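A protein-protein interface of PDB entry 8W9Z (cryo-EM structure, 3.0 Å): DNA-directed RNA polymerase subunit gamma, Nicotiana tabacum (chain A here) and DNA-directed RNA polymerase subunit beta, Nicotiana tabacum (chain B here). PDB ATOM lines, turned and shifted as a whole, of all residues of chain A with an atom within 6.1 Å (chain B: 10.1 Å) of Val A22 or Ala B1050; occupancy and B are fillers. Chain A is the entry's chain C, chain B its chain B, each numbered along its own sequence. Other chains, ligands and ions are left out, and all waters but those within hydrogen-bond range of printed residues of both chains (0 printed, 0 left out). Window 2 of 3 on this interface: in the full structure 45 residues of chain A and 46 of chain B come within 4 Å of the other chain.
The backbone carbonyl oxygen (O) of Gly A20 lies within hydrogen-bond range of the backbone NH (N) of Glu B1052, at 2.8 Å.
The backbone carbonyl oxygen of Leu B1046 sits close to the backbone NH of Leu B1051 (3.4 Å). The side-chain amide nitrogen of Gln A26 sits close to the indole nitrogen of Trp A30 (3.1 Å). The side-chain amide nitrogen of Asn B1054 sits at hydrogen-bond distance from the side-chain carboxylate of Glu B1052 (2.8 Å).
CA of Leu B1051 touches O of Gly A20 (3.6 Å). CG2 of Val A22 touches CB of Ala B1050, at 3.7 Å. Glu B1052 touches Val A22 (CB to CG1, 3.8 Å). CH2 of Trp A30 touches CB of Arg B1047, 3.5 Å away. Pro A277 touches Arg B1047 (CG to O, 3.6 Å).
Val A22 touches two residues of chain B. Of chain A, only Val A22 comes within 4 Å of Ala B1050. No residue of chain B comes within 4 Å of Ser A21. No residue of chain B comes within 4 Å of Trp A270. Printed residues of chain A within 4 Å of Leu B1051: Gly A20. Of the printed residues of chain A, Glu B1052 touches Gly A20 (2.8 Å) and Val A22 (3.8 Å). The nearest residue of chain B that does not touch Val A22 is Leu B1051 (4.1 Å). The nearest residue of chain A that does not touch Ala B1050 is Ser A21 (4.05 Å). The nearest printed residue of chain B that does not touch Trp A30 is Glu B1052 (4.1 Å).
Printed residues of chain A that touch a printed residue of chain B: Gly A20, Val A22, Trp A30 and Pro A277. Hydrophobic or aromatic side chains of chain A that line the printed part of chain B: Val A22, Trp A30 and Pro A277. Along chain B the printed residues that touch a printed residue of chain A span positions 1047 to 1052. Among the printed residues, 6 pairs touch across the chains.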
ATOM      1  N   GLY A  20      -1.810  15.168 -10.045  1.00  0.00           N
ATOM      2  CA  GLY A  20      -3.058  15.894 -10.196  1.00  0.00           C
ATOM      3  C   GLY A  20      -2.878  17.085 -11.108  1.00  0.00           C
ATOM      4  O   GLY A  20      -1.757  17.474 -11.450  1.00  0.00           O
ATOM      5  N   SER A  21      -4.010  17.664 -11.497  1.00  0.00           N
ATOM      6  CA  SER A  21      -4.025  18.842 -12.353  1.00  0.00           C
ATOM      7  C   SER A  21      -3.984  20.096 -11.490  1.00  0.00           C
ATOM      8  O   SER A  21      -4.753  20.225 -10.533  1.00  0.00           O
ATOM      9  CB  SER A  21      -5.267  18.848 -13.245  1.00  0.00           C
ATOM     10  OG  SER A  21      -5.273  19.973 -14.104  1.00  0.00           O
ATOM     11  N   VAL A  22      -3.083  21.019 -11.833  1.00  0.00           N
ATOM     12  CA  VAL A  22      -2.903  22.211 -11.015  1.00  0.00           C
ATOM     13  C   VAL A  22      -4.091  23.152 -11.184  1.00  0.00           C
ATOM     14  O   VAL A  22      -4.845  23.096 -12.164  1.00  0.00           O
ATOM     15  CB  VAL A  22      -1.582  22.917 -11.360  1.00  0.00           C
ATOM     16  CG1 VAL A  22      -0.413  21.964 -11.183  1.00  0.00           C
ATOM     17  CG2 VAL A  22      -1.626  23.460 -12.778  1.00  0.00           C
ATOM     18  N   SER A  23      -4.257  24.031 -10.206  1.00  0.00           N
ATOM     19  CA  SER A  23      -5.293  25.045 -10.116  1.00  0.00           C
ATOM     20  C   SER A  23      -4.738  26.410 -10.505  1.00  0.00           C
ATOM     21  O   SER A  23      -3.547  26.678 -10.322  1.00  0.00           O
ATOM     22  CB  SER A  23      -5.855  25.108  -8.693  1.00  0.00           C
ATOM     23  OG  SER A  23      -6.888  26.071  -8.584  1.00  0.00           O
ATOM     24  N   PRO A  24      -5.574  27.297 -11.055  1.00  0.00           N
ATOM     25  CA  PRO A  24      -5.098  28.650 -11.387  1.00  0.00           C
ATOM     26  C   PRO A  24      -4.605  29.443 -10.187  1.00  0.00           C
ATOM     27  O   PRO A  24      -4.007  30.510 -10.380  1.00  0.00           O
ATOM     28  CB  PRO A  24      -6.330  29.311 -12.020  1.00  0.00           C
ATOM     29  CG  PRO A  24      -7.133  28.172 -12.547  1.00  0.00           C
ATOM     30  CD  PRO A  24      -6.930  27.048 -11.573  1.00  0.00           C
ATOM     31  N   GLN A  26      -2.817  27.730  -7.469  1.00  0.00           N
ATOM     32  CA  GLN A  26      -1.578  27.087  -7.050  1.00  0.00           C
ATOM     33  C   GLN A  26      -0.427  27.374  -8.007  1.00  0.00           C
ATOM     34  O   GLN A  26       0.736  27.289  -7.599  1.00  0.00           O
ATOM     35  CB  GLN A  26      -1.796  25.577  -6.918  1.00  0.00           C
ATOM     36  CG  GLN A  26      -0.768  24.856  -6.057  1.00  0.00           C
ATOM     37  CD  GLN A  26       0.451  24.410  -6.840  1.00  0.00           C
ATOM     38  OE1 GLN A  26       0.449  24.415  -8.071  1.00  0.00           O
ATOM     39  NE2 GLN A  26       1.503  24.023  -6.127  1.00  0.00           N
ATOM     40  N   ILE A  27      -0.725  27.718  -9.263  1.00  0.00           N
ATOM     41  CA  ILE A  27       0.331  28.000 -10.232  1.00  0.00           C
ATOM     42  C   ILE A  27       1.144  29.215  -9.808  1.00  0.00           C
ATOM     43  O   ILE A  27       2.340  29.311 -10.113  1.00  0.00           O
ATOM     44  CB  ILE A  27      -0.277  28.177 -11.639  1.00  0.00           C
ATOM     45  CG1 ILE A  27       0.813  28.462 -12.674  1.00  0.00           C
ATOM     46  CG2 ILE A  27      -1.318  29.284 -11.641  1.00  0.00           C
ATOM     47  CD1 ILE A  27       1.839  27.363 -12.798  1.00  0.00           C
ATOM     48  N   TRP A  30       4.577  28.972  -7.487  1.00  0.00           N
ATOM     49  CA  TRP A  30       5.862  28.512  -7.999  1.00  0.00           C
ATOM     50  C   TRP A  30       6.758  29.666  -8.439  1.00  0.00           C
ATOM     51  O   TRP A  30       7.930  29.726  -8.055  1.00  0.00           O
ATOM     52  CB  TRP A  30       5.646  27.545  -9.167  1.00  0.00           C
ATOM     53  CG  TRP A  30       4.966  26.272  -8.776  1.00  0.00           C
ATOM     54  CD1 TRP A  30       4.828  25.771  -7.517  1.00  0.00           C
ATOM     55  CD2 TRP A  30       4.323  25.340  -9.653  1.00  0.00           C
ATOM     56  NE1 TRP A  30       4.141  24.582  -7.554  1.00  0.00           N
ATOM     57  CE2 TRP A  30       3.820  24.295  -8.854  1.00  0.00           C
ATOM     58  CE3 TRP A  30       4.126  25.287 -11.036  1.00  0.00           C
ATOM     59  CZ2 TRP A  30       3.132  23.211  -9.392  1.00  0.00           C
ATOM     60  CZ3 TRP A  30       3.443  24.210 -11.567  1.00  0.00           C
ATOM     61  CH2 TRP A  30       2.954  23.187 -10.746  1.00  0.00           C
ATOM     62  N   TRP A 124      -4.641  17.646 -24.824  1.00  0.00           N
ATOM     63  CA  TRP A 124      -5.143  16.280 -24.738  1.00  0.00           C
ATOM     64  C   TRP A 124      -6.416  16.166 -23.910  1.00  0.00           C
ATOM     65  O   TRP A 124      -6.689  15.100 -23.340  1.00  0.00           O
ATOM     66  CB  TRP A 124      -4.062  15.342 -24.194  1.00  0.00           C
ATOM     67  CG  TRP A 124      -3.145  15.945 -23.177  1.00  0.00           C
ATOM     68  CD1 TRP A 124      -1.889  16.428 -23.393  1.00  0.00           C
ATOM     69  CD2 TRP A 124      -3.400  16.107 -21.777  1.00  0.00           C
ATOM     70  NE1 TRP A 124      -1.349  16.891 -22.219  1.00  0.00           N
ATOM     71  CE2 TRP A 124      -2.257  16.705 -21.210  1.00  0.00           C
ATOM     72  CE3 TRP A 124      -4.486  15.812 -20.948  1.00  0.00           C
ATOM     73  CZ2 TRP A 124      -2.169  17.011 -19.854  1.00  0.00           C
ATOM     74  CZ3 TRP A 124      -4.395  16.114 -19.602  1.00  0.00           C
ATOM     75  CH2 TRP A 124      -3.246  16.710 -19.069  1.00  0.00           C
ATOM     76  N   TRP A 270     -10.539  23.218 -14.027  1.00  0.00           N
ATOM     77  CA  TRP A 270      -9.101  23.418 -14.138  1.00  0.00           C
ATOM     78  C   TRP A 270      -8.528  22.865 -15.435  1.00  0.00           C
ATOM     79  O   TRP A 270      -7.320  22.985 -15.663  1.00  0.00           O
ATOM     80  CB  TRP A 270      -8.387  22.773 -12.948  1.00  0.00           C
ATOM     81  CG  TRP A 270      -8.748  23.376 -11.628  1.00  0.00           C
ATOM     82  CD1 TRP A 270      -9.366  24.572 -11.417  1.00  0.00           C
ATOM     83  CD2 TRP A 270      -8.516  22.809 -10.333  1.00  0.00           C
ATOM     84  NE1 TRP A 270      -9.530  24.788 -10.069  1.00  0.00           N
ATOM     85  CE2 TRP A 270      -9.018  23.719  -9.384  1.00  0.00           C
ATOM     86  CE3 TRP A 270      -7.932  21.620  -9.885  1.00  0.00           C
ATOM     87  CZ2 TRP A 270      -8.955  23.479  -8.013  1.00  0.00           C
ATOM     88  CZ3 TRP A 270      -7.870  21.384  -8.524  1.00  0.00           C
ATOM     89  CH2 TRP A 270      -8.379  22.309  -7.605  1.00  0.00           C
ATOM     90  N   LEU A 273      -6.565  26.463 -19.361  1.00  0.00           N
ATOM     91  CA  LEU A 273      -5.358  27.121 -18.863  1.00  0.00           C
ATOM     92  C   LEU A 273      -5.611  28.624 -18.809  1.00  0.00           C
ATOM     93  O   LEU A 273      -5.403  29.345 -19.785  1.00  0.00           O
ATOM     94  CB  LEU A 273      -4.152  26.786 -19.732  1.00  0.00           C
ATOM     95  CG  LEU A 273      -3.546  25.386 -19.599  1.00  0.00           C
ATOM     96  CD1 LEU A 273      -4.372  24.347 -20.342  1.00  0.00           C
ATOM     97  CD2 LEU A 273      -2.107  25.379 -20.088  1.00  0.00           C
ATOM     98  N   PRO A 277       2.316  27.807 -17.333  1.00  0.00           N
ATOM     99  CA  PRO A 277       3.644  27.721 -16.717  1.00  0.00           C
ATOM    100  C   PRO A 277       4.748  27.919 -17.745  1.00  0.00           C
ATOM    101  O   PRO A 277       4.536  27.829 -18.956  1.00  0.00           O
ATOM    102  CB  PRO A 277       3.682  26.301 -16.135  1.00  0.00           C
ATOM    103  CG  PRO A 277       2.251  25.836 -16.126  1.00  0.00           C
ATOM    104  CD  PRO A 277       1.602  26.522 -17.282  1.00  0.00           C
ATOM    105  N   LEU B1042      12.363  15.639 -13.623  1.00  0.00           N
ATOM    106  CA  LEU B1042      11.089  15.089 -14.071  1.00  0.00           C
ATOM    107  C   LEU B1042       9.915  15.909 -13.555  1.00  0.00           C
ATOM    108  O   LEU B1042       8.964  16.174 -14.300  1.00  0.00           O
ATOM    109  CB  LEU B1042      10.963  13.632 -13.625  1.00  0.00           C
ATOM    110  CG  LEU B1042       9.693  12.900 -14.062  1.00  0.00           C
ATOM    111  CD1 LEU B1042       9.580  12.882 -15.577  1.00  0.00           C
ATOM    112  CD2 LEU B1042       9.668  11.486 -13.502  1.00  0.00           C
ATOM    113  N   VAL B1043       9.962  16.332 -12.288  1.00  0.00           N
ATOM    114  CA  VAL B1043       8.838  17.087 -11.747  1.00  0.00           C
ATOM    115  C   VAL B1043       8.757  18.463 -12.393  1.00  0.00           C
ATOM    116  O   VAL B1043       7.656  18.972 -12.631  1.00  0.00           O
ATOM    117  CB  VAL B1043       8.914  17.170 -10.209  1.00  0.00           C
ATOM    118  CG1 VAL B1043      10.073  18.035  -9.755  1.00  0.00           C
ATOM    119  CG2 VAL B1043       7.602  17.694  -9.640  1.00  0.00           C
ATOM    120  N   ARG B1044       9.898  19.073 -12.730  1.00  0.00           N
ATOM    121  CA  ARG B1044       9.862  20.348 -13.439  1.00  0.00           C
ATOM    122  C   ARG B1044       9.293  20.176 -14.842  1.00  0.00           C
ATOM    123  O   ARG B1044       8.441  20.962 -15.281  1.00  0.00           O
ATOM    124  CB  ARG B1044      11.261  20.963 -13.498  1.00  0.00           C
ATOM    125  CG  ARG B1044      11.818  21.400 -12.154  1.00  0.00           C
ATOM    126  CD  ARG B1044      10.922  22.420 -11.481  1.00  0.00           C
ATOM    127  NE  ARG B1044      11.522  22.944 -10.257  1.00  0.00           N
ATOM    128  CZ  ARG B1044      11.383  22.387  -9.060  1.00  0.00           C
ATOM    129  NH1 ARG B1044      10.661  21.284  -8.918  1.00  0.00           N
ATOM    130  NH2 ARG B1044      11.965  22.933  -8.001  1.00  0.00           N
ATOM    131  N   GLU B1045       9.749  19.147 -15.562  1.00  0.00           N
ATOM    132  CA  GLU B1045       9.249  18.912 -16.912  1.00  0.00           C
ATOM    133  C   GLU B1045       7.760  18.592 -16.910  1.00  0.00           C
ATOM    134  O   GLU B1045       7.054  18.921 -17.870  1.00  0.00           O
ATOM    135  CB  GLU B1045      10.044  17.785 -17.574  1.00  0.00           C
ATOM    136  CG  GLU B1045       9.826  17.651 -19.077  1.00  0.00           C
ATOM    137  CD  GLU B1045       8.643  16.768 -19.428  1.00  0.00           C
ATOM    138  OE1 GLU B1045       8.178  16.015 -18.549  1.00  0.00           O
ATOM    139  OE2 GLU B1045       8.179  16.830 -20.587  1.00  0.00           O
ATOM    140  N   LEU B1046       7.262  17.958 -15.846  1.00  0.00           N
ATOM    141  CA  LEU B1046       5.843  17.627 -15.794  1.00  0.00           C
ATOM    142  C   LEU B1046       4.997  18.818 -15.358  1.00  0.00           C
ATOM    143  O   LEU B1046       3.889  19.011 -15.871  1.00  0.00           O
ATOM    144  CB  LEU B1046       5.611  16.434 -14.867  1.00  0.00           C
ATOM    145  CG  LEU B1046       6.042  15.083 -15.439  1.00  0.00           C
ATOM    146  CD1 LEU B1046       5.635  13.947 -14.519  1.00  0.00           C
ATOM    147  CD2 LEU B1046       5.460  14.883 -16.829  1.00  0.00           C
ATOM    148  N   ARG B1047       5.491  19.632 -14.422  1.00  0.00           N
ATOM    149  CA  ARG B1047       4.746  20.812 -14.008  1.00  0.00           C
ATOM    150  C   ARG B1047       4.810  21.933 -15.033  1.00  0.00           C
ATOM    151  O   ARG B1047       4.012  22.872 -14.949  1.00  0.00           O
ATOM    152  CB  ARG B1047       5.249  21.318 -12.655  1.00  0.00           C
ATOM    153  CG  ARG B1047       6.617  21.966 -12.682  1.00  0.00           C
ATOM    154  CD  ARG B1047       6.956  22.549 -11.321  1.00  0.00           C
ATOM    155  NE  ARG B1047       6.810  21.567 -10.253  1.00  0.00           N
ATOM    156  CZ  ARG B1047       7.005  21.832  -8.965  1.00  0.00           C
ATOM    157  NH1 ARG B1047       6.849  20.878  -8.058  1.00  0.00           N
ATOM    158  NH2 ARG B1047       7.355  23.052  -8.583  1.00  0.00           N
ATOM    159  N   SER B1048       5.736  21.860 -15.992  1.00  0.00           N
ATOM    160  CA  SER B1048       5.678  22.764 -17.133  1.00  0.00           C
ATOM    161  C   SER B1048       4.453  22.525 -18.006  1.00  0.00           C
ATOM    162  O   SER B1048       4.160  23.355 -18.873  1.00  0.00           O
ATOM    163  CB  SER B1048       6.943  22.626 -17.979  1.00  0.00           C
ATOM    164  OG  SER B1048       6.899  23.483 -19.106  1.00  0.00           O
ATOM    165  N   LEU B1049       3.738  21.419 -17.800  1.00  0.00           N
ATOM    166  CA  LEU B1049       2.540  21.087 -18.561  1.00  0.00           C
ATOM    167  C   LEU B1049       1.319  20.972 -17.653  1.00  0.00           C
ATOM    168  O   LEU B1049       0.388  20.221 -17.948  1.00  0.00           O
ATOM    169  CB  LEU B1049       2.747  19.795 -19.348  1.00  0.00           C
ATOM    170  CG  LEU B1049       4.001  19.758 -20.224  1.00  0.00           C
ATOM    171  CD1 LEU B1049       4.210  18.373 -20.809  1.00  0.00           C
ATOM    172  CD2 LEU B1049       3.917  20.803 -21.326  1.00  0.00           C
ATOM    173  N   ALA B1050       1.325  21.709 -16.539  1.00  0.00           N
ATOM    174  CA  ALA B1050       0.208  21.747 -15.591  1.00  0.00           C
ATOM    175  C   ALA B1050      -0.069  20.368 -14.991  1.00  0.00           C
ATOM    176  O   ALA B1050      -1.186  19.847 -15.057  1.00  0.00           O
ATOM    177  CB  ALA B1050      -1.051  22.325 -16.243  1.00  0.00           C
ATOM    178  N   LEU B1051       0.964  19.776 -14.394  1.00  0.00           N
ATOM    179  CA  LEU B1051       0.859  18.488 -13.716  1.00  0.00           C
ATOM    180  C   LEU B1051       1.640  18.564 -12.413  1.00  0.00           C
ATOM    181  O   LEU B1051       2.833  18.878 -12.421  1.00  0.00           O
ATOM    182  CB  LEU B1051       1.388  17.352 -14.595  1.00  0.00           C
ATOM    183  CG  LEU B1051       0.659  17.091 -15.914  1.00  0.00           C
ATOM    184  CD1 LEU B1051       1.380  16.023 -16.720  1.00  0.00           C
ATOM    185  CD2 LEU B1051      -0.782  16.688 -15.660  1.00  0.00           C
ATOM    186  N   GLU B1052       0.976  18.266 -11.301  1.00  0.00           N
ATOM    187  CA  GLU B1052       1.574  18.388  -9.979  1.00  0.00           C
ATOM    188  C   GLU B1052       2.023  17.023  -9.471  1.00  0.00           C
ATOM    189  O   GLU B1052       1.313  16.025  -9.629  1.00  0.00           O
ATOM    190  CB  GLU B1052       0.584  19.013  -8.994  1.00  0.00           C
ATOM    191  CG  GLU B1052       1.227  19.855  -7.902  1.00  0.00           C
ATOM    192  CD  GLU B1052       1.907  19.021  -6.835  1.00  0.00           C
ATOM    193  OE1 GLU B1052       1.474  17.872  -6.606  1.00  0.00           O
ATOM    194  OE2 GLU B1052       2.878  19.516  -6.225  1.00  0.00           O
ATOM    195  N   LEU B1053       3.207  16.987  -8.861  1.00  0.00           N
ATOM    196  CA  LEU B1053       3.752  15.779  -8.258  1.00  0.00           C
ATOM    197  C   LEU B1053       4.228  16.079  -6.845  1.00  0.00           C
ATOM    198  O   LEU B1053       4.749  17.164  -6.573  1.00  0.00           O
ATOM    199  CB  LEU B1053       4.917  15.209  -9.073  1.00  0.00           C
ATOM    200  CG  LEU B1053       4.593  14.500 -10.388  1.00  0.00           C
ATOM    201  CD1 LEU B1053       5.829  13.791 -10.907  1.00  0.00           C
ATOM    202  CD2 LEU B1053       3.449  13.522 -10.202  1.00  0.00           C
ATOM    203  N   ASN B1054       4.048  15.109  -5.952  1.00  0.00           N
ATOM    204  CA  ASN B1054       4.505  15.217  -4.576  1.00  0.00           C
ATOM    205  C   ASN B1054       5.034  13.866  -4.119  1.00  0.00           C
ATOM    206  O   ASN B1054       4.545  12.817  -4.542  1.00  0.00           O
ATOM    207  CB  ASN B1054       3.383  15.689  -3.641  1.00  0.00           C
ATOM    208  CG  ASN B1054       3.013  17.142  -3.860  1.00  0.00           C
ATOM    209  OD1 ASN B1054       3.882  17.998  -4.023  1.00  0.00           O
ATOM    210  ND2 ASN B1054       1.717  17.428  -3.867  1.00  0.00           N
